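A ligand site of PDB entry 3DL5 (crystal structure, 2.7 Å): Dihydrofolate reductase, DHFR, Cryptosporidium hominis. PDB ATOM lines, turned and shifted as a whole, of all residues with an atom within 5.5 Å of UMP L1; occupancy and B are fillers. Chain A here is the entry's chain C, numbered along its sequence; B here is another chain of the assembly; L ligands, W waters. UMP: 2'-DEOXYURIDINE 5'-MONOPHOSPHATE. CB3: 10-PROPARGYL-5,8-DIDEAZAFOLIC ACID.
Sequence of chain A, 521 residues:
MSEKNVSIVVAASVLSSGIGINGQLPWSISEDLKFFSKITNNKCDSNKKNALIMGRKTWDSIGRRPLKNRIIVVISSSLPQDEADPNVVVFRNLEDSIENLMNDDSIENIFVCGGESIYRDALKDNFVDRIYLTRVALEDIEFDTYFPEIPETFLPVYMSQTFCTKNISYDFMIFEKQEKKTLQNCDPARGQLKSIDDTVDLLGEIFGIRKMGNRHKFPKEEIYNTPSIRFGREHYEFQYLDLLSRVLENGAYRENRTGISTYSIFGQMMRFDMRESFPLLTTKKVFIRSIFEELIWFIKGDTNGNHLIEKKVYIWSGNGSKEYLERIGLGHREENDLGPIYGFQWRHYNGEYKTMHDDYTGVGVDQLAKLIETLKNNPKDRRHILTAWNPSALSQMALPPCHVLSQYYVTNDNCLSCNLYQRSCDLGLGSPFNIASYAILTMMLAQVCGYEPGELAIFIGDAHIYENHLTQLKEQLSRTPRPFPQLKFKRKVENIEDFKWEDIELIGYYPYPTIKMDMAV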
ATOM      1  N   ARG A 257      15.898  23.235 -24.781  1.00  0.00           N
ATOM      2  CA  ARG A 257      17.252  23.523 -24.304  1.00  0.00           C
ATOM      3  C   ARG A 257      17.982  22.394 -23.558  1.00  0.00           C
ATOM      4  O   ARG A 257      19.207  22.300 -23.622  1.00  0.00           O
ATOM      5  CB  ARG A 257      17.254  24.766 -23.414  1.00  0.00           C
ATOM      6  CG  ARG A 257      16.147  24.778 -22.363  1.00  0.00           C
ATOM      7  CD  ARG A 257      16.467  25.728 -21.194  1.00  0.00           C
ATOM      8  NE  ARG A 257      17.378  25.100 -20.239  1.00  0.00           N
ATOM      9  CZ  ARG A 257      17.011  24.597 -19.061  1.00  0.00           C
ATOM     10  NH1 ARG A 257      15.748  24.652 -18.678  1.00  0.00           N
ATOM     11  NH2 ARG A 257      17.902  24.015 -18.283  1.00  0.00           N
ATOM     12  N   TRP A 316      18.700  22.251  -6.420  1.00  0.00           N
ATOM     13  CA  TRP A 316      19.277  23.292  -7.257  1.00  0.00           C
ATOM     14  C   TRP A 316      20.719  23.052  -7.676  1.00  0.00           C
ATOM     15  O   TRP A 316      21.322  23.903  -8.313  1.00  0.00           O
ATOM     16  CB  TRP A 316      19.167  24.668  -6.588  1.00  0.00           C
ATOM     17  CG  TRP A 316      17.800  25.280  -6.696  1.00  0.00           C
ATOM     18  CD1 TRP A 316      16.773  25.177  -5.800  1.00  0.00           C
ATOM     19  CD2 TRP A 316      17.292  26.051  -7.799  1.00  0.00           C
ATOM     20  NE1 TRP A 316      15.667  25.849  -6.267  1.00  0.00           N
ATOM     21  CE2 TRP A 316      15.954  26.390  -7.492  1.00  0.00           C
ATOM     22  CE3 TRP A 316      17.844  26.492  -9.011  1.00  0.00           C
ATOM     23  CZ2 TRP A 316      15.148  27.153  -8.352  1.00  0.00           C
ATOM     24  CZ3 TRP A 316      17.043  27.252  -9.883  1.00  0.00           C
ATOM     25  CH2 TRP A 316      15.711  27.565  -9.543  1.00  0.00           C
ATOM     26  N   TYR A 342      14.526  33.762  -7.729  1.00  0.00           N
ATOM     27  CA  TYR A 342      13.258  33.920  -7.005  1.00  0.00           C
ATOM     28  C   TYR A 342      13.390  34.685  -5.686  1.00  0.00           C
ATOM     29  O   TYR A 342      12.661  35.657  -5.447  1.00  0.00           O
ATOM     30  CB  TYR A 342      12.700  32.539  -6.702  1.00  0.00           C
ATOM     31  CG  TYR A 342      12.249  31.760  -7.915  1.00  0.00           C
ATOM     32  CD1 TYR A 342      11.126  32.173  -8.658  1.00  0.00           C
ATOM     33  CD2 TYR A 342      12.920  30.615  -8.332  1.00  0.00           C
ATOM     34  CE1 TYR A 342      10.700  31.447  -9.762  1.00  0.00           C
ATOM     35  CE2 TYR A 342      12.502  29.884  -9.432  1.00  0.00           C
ATOM     36  CZ  TYR A 342      11.386  30.313 -10.146  1.00  0.00           C
ATOM     37  OH  TYR A 342      10.963  29.587 -11.233  1.00  0.00           O
ATOM     38  N   LEU A 399      18.499  30.361 -14.085  1.00  0.00           N
ATOM     39  CA  LEU A 399      17.312  29.918 -14.807  1.00  0.00           C
ATOM     40  C   LEU A 399      16.271  31.027 -14.671  1.00  0.00           C
ATOM     41  O   LEU A 399      16.112  31.591 -13.600  1.00  0.00           O
ATOM     42  CB  LEU A 399      16.786  28.642 -14.159  1.00  0.00           C
ATOM     43  CG  LEU A 399      16.297  27.468 -15.012  1.00  0.00           C
ATOM     44  CD1 LEU A 399      17.280  27.174 -16.142  1.00  0.00           C
ATOM     45  CD2 LEU A 399      16.131  26.258 -14.105  1.00  0.00           C
ATOM     46  N   PRO A 400      15.586  31.373 -15.764  1.00  0.00           N
ATOM     47  CA  PRO A 400      14.579  32.422 -15.589  1.00  0.00           C
ATOM     48  C   PRO A 400      13.387  31.803 -14.854  1.00  0.00           C
ATOM     49  O   PRO A 400      13.043  30.648 -15.070  1.00  0.00           O
ATOM     50  CB  PRO A 400      14.269  32.859 -17.026  1.00  0.00           C
ATOM     51  CG  PRO A 400      14.608  31.650 -17.849  1.00  0.00           C
ATOM     52  CD  PRO A 400      15.838  31.086 -17.186  1.00  0.00           C
ATOM     53  N   CYS A 402      10.089  30.217 -13.416  1.00  0.00           N
ATOM     54  CA  CYS A 402       9.092  29.375 -14.072  1.00  0.00           C
ATOM     55  C   CYS A 402       7.695  29.654 -13.549  1.00  0.00           C
ATOM     56  O   CYS A 402       6.749  29.818 -14.323  1.00  0.00           O
ATOM     57  CB  CYS A 402       9.444  27.893 -13.892  1.00  0.00           C
ATOM     58  SG  CYS A 402      10.489  27.199 -15.195  1.00  0.00           S
ATOM     59  N   HIS A 403       7.563  29.704 -12.229  1.00  0.00           N
ATOM     60  CA  HIS A 403       6.351  30.222 -11.600  1.00  0.00           C
ATOM     61  C   HIS A 403       6.427  31.722 -11.389  1.00  0.00           C
ATOM     62  O   HIS A 403       7.105  32.202 -10.479  1.00  0.00           O
ATOM     63  CB  HIS A 403       6.109  29.513 -10.260  1.00  0.00           C
ATOM     64  CG  HIS A 403       7.329  29.419  -9.397  1.00  0.00           C
ATOM     65  ND1 HIS A 403       7.395  29.967  -8.142  1.00  0.00           N
ATOM     66  CD2 HIS A 403       8.528  28.831  -9.619  1.00  0.00           C
ATOM     67  CE1 HIS A 403       8.582  29.727  -7.620  1.00  0.00           C
ATOM     68  NE2 HIS A 403       9.288  29.037  -8.494  1.00  0.00           N
ATOM     69  N   GLN A 422       2.235  29.918 -14.020  1.00  0.00           N
ATOM     70  CA  GLN A 422       3.525  29.258 -14.134  1.00  0.00           C
ATOM     71  C   GLN A 422       3.874  28.980 -15.611  1.00  0.00           C
ATOM     72  O   GLN A 422       3.389  28.020 -16.211  1.00  0.00           O
ATOM     73  CB  GLN A 422       3.479  27.974 -13.295  1.00  0.00           C
ATOM     74  CG  GLN A 422       4.529  26.964 -13.654  1.00  0.00           C
ATOM     75  CD  GLN A 422       4.707  25.876 -12.612  1.00  0.00           C
ATOM     76  OE1 GLN A 422       5.833  25.449 -12.349  1.00  0.00           O
ATOM     77  NE2 GLN A 422       3.599  25.416 -12.031  1.00  0.00           N
ATOM     78  N   ARG A 423       4.720  29.841 -16.191  1.00  0.00           N
ATOM     79  CA  ARG A 423       5.142  29.733 -17.595  1.00  0.00           C
ATOM     80  C   ARG A 423       5.606  28.347 -18.054  1.00  0.00           C
ATOM     81  O   ARG A 423       5.240  27.862 -19.128  1.00  0.00           O
ATOM     82  CB  ARG A 423       6.264  30.742 -17.884  1.00  0.00           C
ATOM     83  CG  ARG A 423       7.636  30.278 -17.430  1.00  0.00           C
ATOM     84  CD  ARG A 423       8.709  31.192 -17.972  1.00  0.00           C
ATOM     85  NE  ARG A 423      10.035  30.763 -17.537  1.00  0.00           N
ATOM     86  CZ  ARG A 423      10.704  29.723 -18.026  1.00  0.00           C
ATOM     87  NH1 ARG A 423      10.194  28.969 -19.002  1.00  0.00           N
ATOM     88  NH2 ARG A 423      11.884  29.410 -17.522  1.00  0.00           N
ATOM     89  N   SER A 424       6.443  27.701 -17.244  1.00  0.00           N
ATOM     90  CA  SER A 424       6.951  26.387 -17.609  1.00  0.00           C
ATOM     91  C   SER A 424       6.757  25.438 -16.434  1.00  0.00           C
ATOM     92  O   SER A 424       7.140  25.740 -15.305  1.00  0.00           O
ATOM     93  CB  SER A 424       8.434  26.488 -17.972  1.00  0.00           C
ATOM     94  OG  SER A 424       8.937  25.224 -18.370  1.00  0.00           O
ATOM     95  N   CYS A 425       6.158  24.297 -16.703  1.00  0.00           N
ATOM     96  CA  CYS A 425       5.900  23.353 -15.639  1.00  0.00           C
ATOM     97  C   CYS A 425       6.189  21.903 -15.981  1.00  0.00           C
ATOM     98  O   CYS A 425       5.536  21.294 -16.842  1.00  0.00           O
ATOM     99  CB  CYS A 425       4.446  23.478 -15.180  1.00  0.00           C
ATOM    100  SG  CYS A 425       3.963  22.256 -13.949  1.00  0.00           S
ATOM    101  N   ASP A 426       7.192  21.358 -15.302  1.00  0.00           N
ATOM    102  CA  ASP A 426       7.586  19.968 -15.463  1.00  0.00           C
ATOM    103  C   ASP A 426       6.600  19.189 -14.599  1.00  0.00           C
ATOM    104  O   ASP A 426       6.765  19.108 -13.386  1.00  0.00           O
ATOM    105  CB  ASP A 426       9.017  19.798 -14.965  1.00  0.00           C
ATOM    106  CG  ASP A 426       9.446  18.356 -14.911  1.00  0.00           C
ATOM    107  OD1 ASP A 426      10.650  18.122 -14.657  1.00  0.00           O
ATOM    108  OD2 ASP A 426       8.600  17.455 -15.099  1.00  0.00           O
ATOM    109  N   GLY A 430       8.391  19.048 -11.154  1.00  0.00           N
ATOM    110  CA  GLY A 430       8.338  20.418 -10.697  1.00  0.00           C
ATOM    111  C   GLY A 430       7.000  20.631 -10.046  1.00  0.00           C
ATOM    112  O   GLY A 430       6.918  21.037  -8.884  1.00  0.00           O
ATOM    113  N   SER A 431       5.938  20.358 -10.794  1.00  0.00           N
ATOM    114  CA  SER A 431       4.584  20.572 -10.329  1.00  0.00           C
ATOM    115  C   SER A 431       4.238  20.119  -8.918  1.00  0.00           C
ATOM    116  O   SER A 431       3.722  20.908  -8.126  1.00  0.00           O
ATOM    117  CB  SER A 431       3.612  19.974 -11.342  1.00  0.00           C
ATOM    118  OG  SER A 431       2.375  20.639 -11.250  1.00  0.00           O
ATOM    119  N   ASN A 434       5.729  22.549  -6.741  1.00  0.00           N
ATOM    120  CA  ASN A 434       5.082  23.856  -6.843  1.00  0.00           C
ATOM    121  C   ASN A 434       3.762  23.956  -6.111  1.00  0.00           C
ATOM    122  O   ASN A 434       3.440  24.989  -5.516  1.00  0.00           O
ATOM    123  CB  ASN A 434       4.857  24.245  -8.305  1.00  0.00           C
ATOM    124  CG  ASN A 434       6.121  24.569  -9.017  1.00  0.00           C
ATOM    125  OD1 ASN A 434       6.527  23.862  -9.943  1.00  0.00           O
ATOM    126  ND2 ASN A 434       6.784  25.650  -8.598  1.00  0.00           N
ATOM    127  N   HIS A 464       4.237  20.285 -19.570  1.00  0.00           N
ATOM    128  CA  HIS A 464       4.882  19.173 -20.263  1.00  0.00           C
ATOM    129  C   HIS A 464       5.325  17.990 -19.420  1.00  0.00           C
ATOM    130  O   HIS A 464       5.386  18.053 -18.186  1.00  0.00           O
ATOM    131  CB  HIS A 464       6.093  19.709 -21.028  1.00  0.00           C
ATOM    132  CG  HIS A 464       7.017  20.539 -20.198  1.00  0.00           C
ATOM    133  ND1 HIS A 464       6.782  21.873 -19.917  1.00  0.00           N
ATOM    134  CD2 HIS A 464       8.181  20.232 -19.561  1.00  0.00           C
ATOM    135  CE1 HIS A 464       7.760  22.350 -19.169  1.00  0.00           C
ATOM    136  NE2 HIS A 464       8.621  21.373 -18.940  1.00  0.00           N
ATOM    137  N   TYR A 466       8.575  15.297 -19.563  1.00  0.00           N
ATOM    138  CA  TYR A 466       9.811  14.873 -20.206  1.00  0.00           C
ATOM    139  C   TYR A 466       9.794  13.385 -20.517  1.00  0.00           C
ATOM    140  O   TYR A 466       9.239  12.590 -19.765  1.00  0.00           O
ATOM    141  CB  TYR A 466      11.012  15.205 -19.319  1.00  0.00           C
ATOM    142  CG  TYR A 466      11.351  16.683 -19.269  1.00  0.00           C
ATOM    143  CD1 TYR A 466      12.319  17.225 -20.096  1.00  0.00           C
ATOM    144  CD2 TYR A 466      10.688  17.539 -18.392  1.00  0.00           C
ATOM    145  CE1 TYR A 466      12.622  18.574 -20.048  1.00  0.00           C
ATOM    146  CE2 TYR A 466      10.986  18.884 -18.337  1.00  0.00           C
ATOM    147  CZ  TYR A 466      11.951  19.394 -19.171  1.00  0.00           C
ATOM    148  OH  TYR A 466      12.262  20.738 -19.119  1.00  0.00           O
ATOM    149  N   ASP B 381      10.992  27.712 -27.654  1.00  0.00           N
ATOM    150  CA  ASP B 381      11.446  28.269 -26.378  1.00  0.00           C
ATOM    151  C   ASP B 381      10.268  28.478 -25.406  1.00  0.00           C
ATOM    152  O   ASP B 381       9.214  28.982 -25.794  1.00  0.00           O
ATOM    153  CB  ASP B 381      12.173  29.596 -26.653  1.00  0.00           C
ATOM    154  CG  ASP B 381      12.589  30.319 -25.387  1.00  0.00           C
ATOM    155  OD1 ASP B 381      13.364  29.737 -24.580  1.00  0.00           O
ATOM    156  OD2 ASP B 381      12.146  31.473 -25.200  1.00  0.00           O
ATOM    157  N   ARG B 382      10.449  28.072 -24.148  1.00  0.00           N
ATOM    158  CA  ARG B 382       9.397  28.205 -23.140  1.00  0.00           C
ATOM    159  C   ARG B 382       9.475  29.508 -22.351  1.00  0.00           C
ATOM    160  O   ARG B 382       8.939  29.608 -21.249  1.00  0.00           O
ATOM    161  CB  ARG B 382       9.461  27.006 -22.172  1.00  0.00           C
ATOM    162  CG  ARG B 382       9.256  25.662 -22.836  1.00  0.00           C
ATOM    163  CD  ARG B 382       9.336  24.495 -21.865  1.00  0.00           C
ATOM    164  NE  ARG B 382      10.688  24.312 -21.327  1.00  0.00           N
ATOM    165  CZ  ARG B 382      11.265  23.128 -21.100  1.00  0.00           C
ATOM    166  NH1 ARG B 382      10.604  22.002 -21.357  1.00  0.00           N
ATOM    167  NH2 ARG B 382      12.495  23.075 -20.621  1.00  0.00           N
ATOM    168  N   ARG B 383       9.994  30.555 -22.977  1.00  0.00           N
ATOM    169  CA  ARG B 383      10.237  31.810 -22.289  1.00  0.00           C
ATOM    170  C   ARG B 383       9.680  33.036 -22.989  1.00  0.00           C
ATOM    171  O   ARG B 383      10.061  34.159 -22.688  1.00  0.00           O
ATOM    172  CB  ARG B 383      11.726  31.991 -22.043  1.00  0.00           C
ATOM    173  CG  ARG B 383      12.211  31.349 -20.802  1.00  0.00           C
ATOM    174  CD  ARG B 383      13.062  30.163 -21.073  1.00  0.00           C
ATOM    175  NE  ARG B 383      14.465  30.534 -21.081  1.00  0.00           N
ATOM    176  CZ  ARG B 383      15.418  29.834 -20.502  1.00  0.00           C
ATOM    177  NH1 ARG B 383      15.131  28.726 -19.856  1.00  0.00           N
ATOM    178  NH2 ARG B 383      16.674  30.250 -20.567  1.00  0.00           N
HETATM  179  N1  UMP L   1      10.334  24.040 -13.689  1.00  0.00           N
HETATM  180  C2  UMP L   1       9.135  23.868 -12.979  1.00  0.00           C
HETATM  181  N3  UMP L   1       8.858  24.679 -11.870  1.00  0.00           N
HETATM  182  C4  UMP L   1       9.856  25.486 -11.303  1.00  0.00           C
HETATM  183  C5  UMP L   1      11.281  25.447 -11.854  1.00  0.00           C
HETATM  184  C6  UMP L   1      11.284  25.125 -13.351  1.00  0.00           C
HETATM  185  O2  UMP L   1       8.279  23.108 -13.425  1.00  0.00           O
HETATM  186  O4  UMP L   1       9.578  26.231 -10.361  1.00  0.00           O
HETATM  187  C1' UMP L   1      10.571  23.276 -14.935  1.00  0.00           C
HETATM  188  C2' UMP L   1       9.863  23.904 -16.132  1.00  0.00           C
HETATM  189  C3' UMP L   1      10.702  23.298 -17.260  1.00  0.00           C
HETATM  190  C4' UMP L   1      12.092  23.590 -16.679  1.00  0.00           C
HETATM  191  O3' UMP L   1      10.496  21.883 -17.348  1.00  0.00           O
HETATM  192  O4' UMP L   1      11.975  23.363 -15.259  1.00  0.00           O
HETATM  193  C5' UMP L   1      12.428  25.055 -16.952  1.00  0.00           C
HETATM  194  O5' UMP L   1      12.935  25.162 -18.278  1.00  0.00           O
HETATM  195  P   UMP L   1      12.559  26.381 -19.257  1.00  0.00           P
HETATM  196  OP1 UMP L   1      13.006  27.705 -18.785  1.00  0.00           O
HETATM  197  OP2 UMP L   1      13.210  25.976 -20.676  1.00  0.00           O
HETATM  198  OP3 UMP L   1      10.965  26.328 -19.477  1.00  0.00           O
HETATM  199  N1  CB3 L   2      14.192  21.795 -14.348  1.00  0.00           N
HETATM  200  C2  CB3 L   2      13.318  20.982 -14.940  1.00  0.00           C
HETATM  201  NA2 CB3 L   2      13.538  20.619 -16.217  1.00  0.00           N
HETATM  202  N3  CB3 L   2      12.239  20.510 -14.282  1.00  0.00           N
HETATM  203  C4  CB3 L   2      12.033  20.872 -13.008  1.00  0.00           C
HETATM  204  O4  CB3 L   2      10.949  20.405 -12.337  1.00  0.00           O
HETATM  205  C4A CB3 L   2      12.923  21.704 -12.377  1.00  0.00           C
HETATM  206  C5  CB3 L   2      12.719  22.085 -11.062  1.00  0.00           C
HETATM  207  C6  CB3 L   2      13.631  22.924 -10.465  1.00  0.00           C
HETATM  208  C7  CB3 L   2      14.725  23.391 -11.155  1.00  0.00           C
HETATM  209  C8  CB3 L   2      14.923  23.007 -12.464  1.00  0.00           C
HETATM  210  C8A CB3 L   2      14.009  22.176 -13.072  1.00  0.00           C
HETATM  211  C9  CB3 L   2      13.445  23.347  -9.039  1.00  0.00           C
HETATM  212  N10 CB3 L   2      12.623  22.407  -8.325  1.00  0.00           N
HETATM  213  C11 CB3 L   2      13.242  18.294  -8.258  1.00  0.00           C
HETATM  214  C12 CB3 L   2      12.062  18.833  -7.788  1.00  0.00           C
HETATM  215  C13 CB3 L   2      11.877  20.197  -7.835  1.00  0.00           C
HETATM  216  C14 CB3 L   2      12.855  21.034  -8.330  1.00  0.00           C
HETATM  217  C15 CB3 L   2      14.047  20.497  -8.773  1.00  0.00           C
HETATM  218  C16 CB3 L   2      14.244  19.125  -8.735  1.00  0.00           C
HETATM  219  C   CB3 L   2      13.434  16.822  -8.151  1.00  0.00           C
HETATM  220  O   CB3 L   2      14.206  16.214  -8.865  1.00  0.00           O
HETATM  221  N   CB3 L   2      12.738  16.254  -7.191  1.00  0.00           N
HETATM  222  CA  CB3 L   2      12.780  14.850  -6.846  1.00  0.00           C
HETATM  223  CB  CB3 L   2      13.060  14.982  -5.372  1.00  0.00           C
HETATM  224  CG  CB3 L   2      14.380  14.370  -4.959  1.00  0.00           C
HETATM  225  CD  CB3 L   2      14.464  14.552  -3.467  1.00  0.00           C
HETATM  226  OE1 CB3 L   2      13.817  15.481  -2.951  1.00  0.00           O
HETATM  227  OE2 CB3 L   2      15.168  13.757  -2.811  1.00  0.00           O
HETATM  228  CT  CB3 L   2      11.443  14.209  -6.949  1.00  0.00           C
HETATM  229  O1  CB3 L   2      11.382  12.968  -7.072  1.00  0.00           O
HETATM  230  O2  CB3 L   2      10.430  14.930  -6.907  1.00  0.00           O
HETATM  231  CP1 CB3 L   2      11.556  22.909  -7.508  1.00  0.00           C
HETATM  232  CP2 CB3 L   2      10.316  22.924  -8.275  1.00  0.00           C
HETATM  233  CP3 CB3 L   2       9.235  22.941  -8.933  1.00  0.00           C
HETATM  234  O   HOH W   1      11.398  26.670  -7.681  1.00  0.00           O
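The guanidinium group (NH2) of Arg 423 lies within salt-bridge range of an oxygen (OP1) of UMP L1 (2.4 Å).
A ring nitrogen (NE2) of His 464 is in hydrogen-bond range of an oxygen (O3') of UMP L1 (2.5 Å).
OG of Ser 424 lies within hydrogen-bond range of OP3 of UMP L1, 2.6 Å away.
An oxygen (OP1) of UMP L1 is in salt-bridge range of the guanidinium group of Arg 383 of chain B, at 2.6 Å.
The guanidinium group (NE) of Arg 382 of chain B lies within salt-bridge range of an oxygen (OP3) of UMP L1, at 2.8 Å.
An oxygen (O3') of UMP L1 lies within hydrogen-bond range of the side-chain hydroxyl of Tyr 466, 2.8 Å away.
O2 of UMP L1 sits at hydrogen-bond distance from N of Asp 426, 2.8 Å away.
An oxygen (OP2) of UMP L1 lies within salt-bridge range of the guanidinium group (NH1) of Arg 257 (3.5 Å).
An oxygen (O4) of UMP L1 lies close to a ring nitrogen (NE2) of His 403 (3.4 Å).
OD1 of Asn 434 lies within hydrogen-bond range of N3 of UMP L1 (3.1 Å).
OE1 of Gln 422 lies within hydrogen-bond range of N3 of UMP L1, at 3.2 Å.
A nitrogen (NA2) of CB3 L2 is in hydrogen-bond range of the side-chain hydroxyl of Tyr 466.
The side-chain carboxylate (OD1) of Asp 426 sits at hydrogen-bond distance from a nitrogen (N3) of CB3 L2 (2.9 Å).
N of Gly 430 sits close to O4 of CB3 L2.
A nitrogen (N1) of CB3 L2 sits close to an oxygen (O4') of UMP L1.
N of Arg 423 sits at hydrogen-bond distance from O of Cys 402, at 2.8 Å.
NE2 of His 464 is in hydrogen-bond range of NH1 of Arg 382 of chain B (3.2 Å).
SG of Cys 402 lies close to O of Ser 424.
The side-chain amide oxygen (OE1) of Gln 422 sits close to the backbone carbonyl oxygen (O) of Ser 424 (3.2 Å).
OD1 of Asp 381 of chain B is in salt-bridge range of NE of Arg 383 of chain B, 3.8 Å away.
The backbone NH of Cys 402 lies within hydrogen-bond range of the side-chain hydroxyl of Tyr 342 (2.4 Å).
OE1 of Gln 422 lies close to OD1 of Asn 434 (3.0 Å).
The side-chain amide oxygen of Asn 434 sits close to the backbone carbonyl oxygen of Gly 430 (3.0 Å).
N1 of UMP L1 sits close to SG of Cys 402.
Tyr 342 touches UMP L1.
CA of Cys 425 touches O2 of UMP L1, 3.3 Å away.
Gly 430 touches UMP L1 (CA to O2, 3.8 Å).
Hydrophobic or aromatic side chains that line UMP L1: His 403, His 464 and Tyr 466.
Within 4 Å of UMP L1: Arg 257, Tyr 342, Cys 402, His 403, Gln 422, Arg 423, Ser 424, Cys 425, Asp 426, Gly 430, Asn 434, His 464, Tyr 466, Arg 382 of chain B and Arg 383 of chain B.
Along chain A the residues within 4 Å of UMP L1 span positions 257 to 466.
Water W1 bridges an oxygen (O4) of UMP L1 (3.3 Å) and a ring nitrogen (NE2) of His 403 (3.3 Å).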
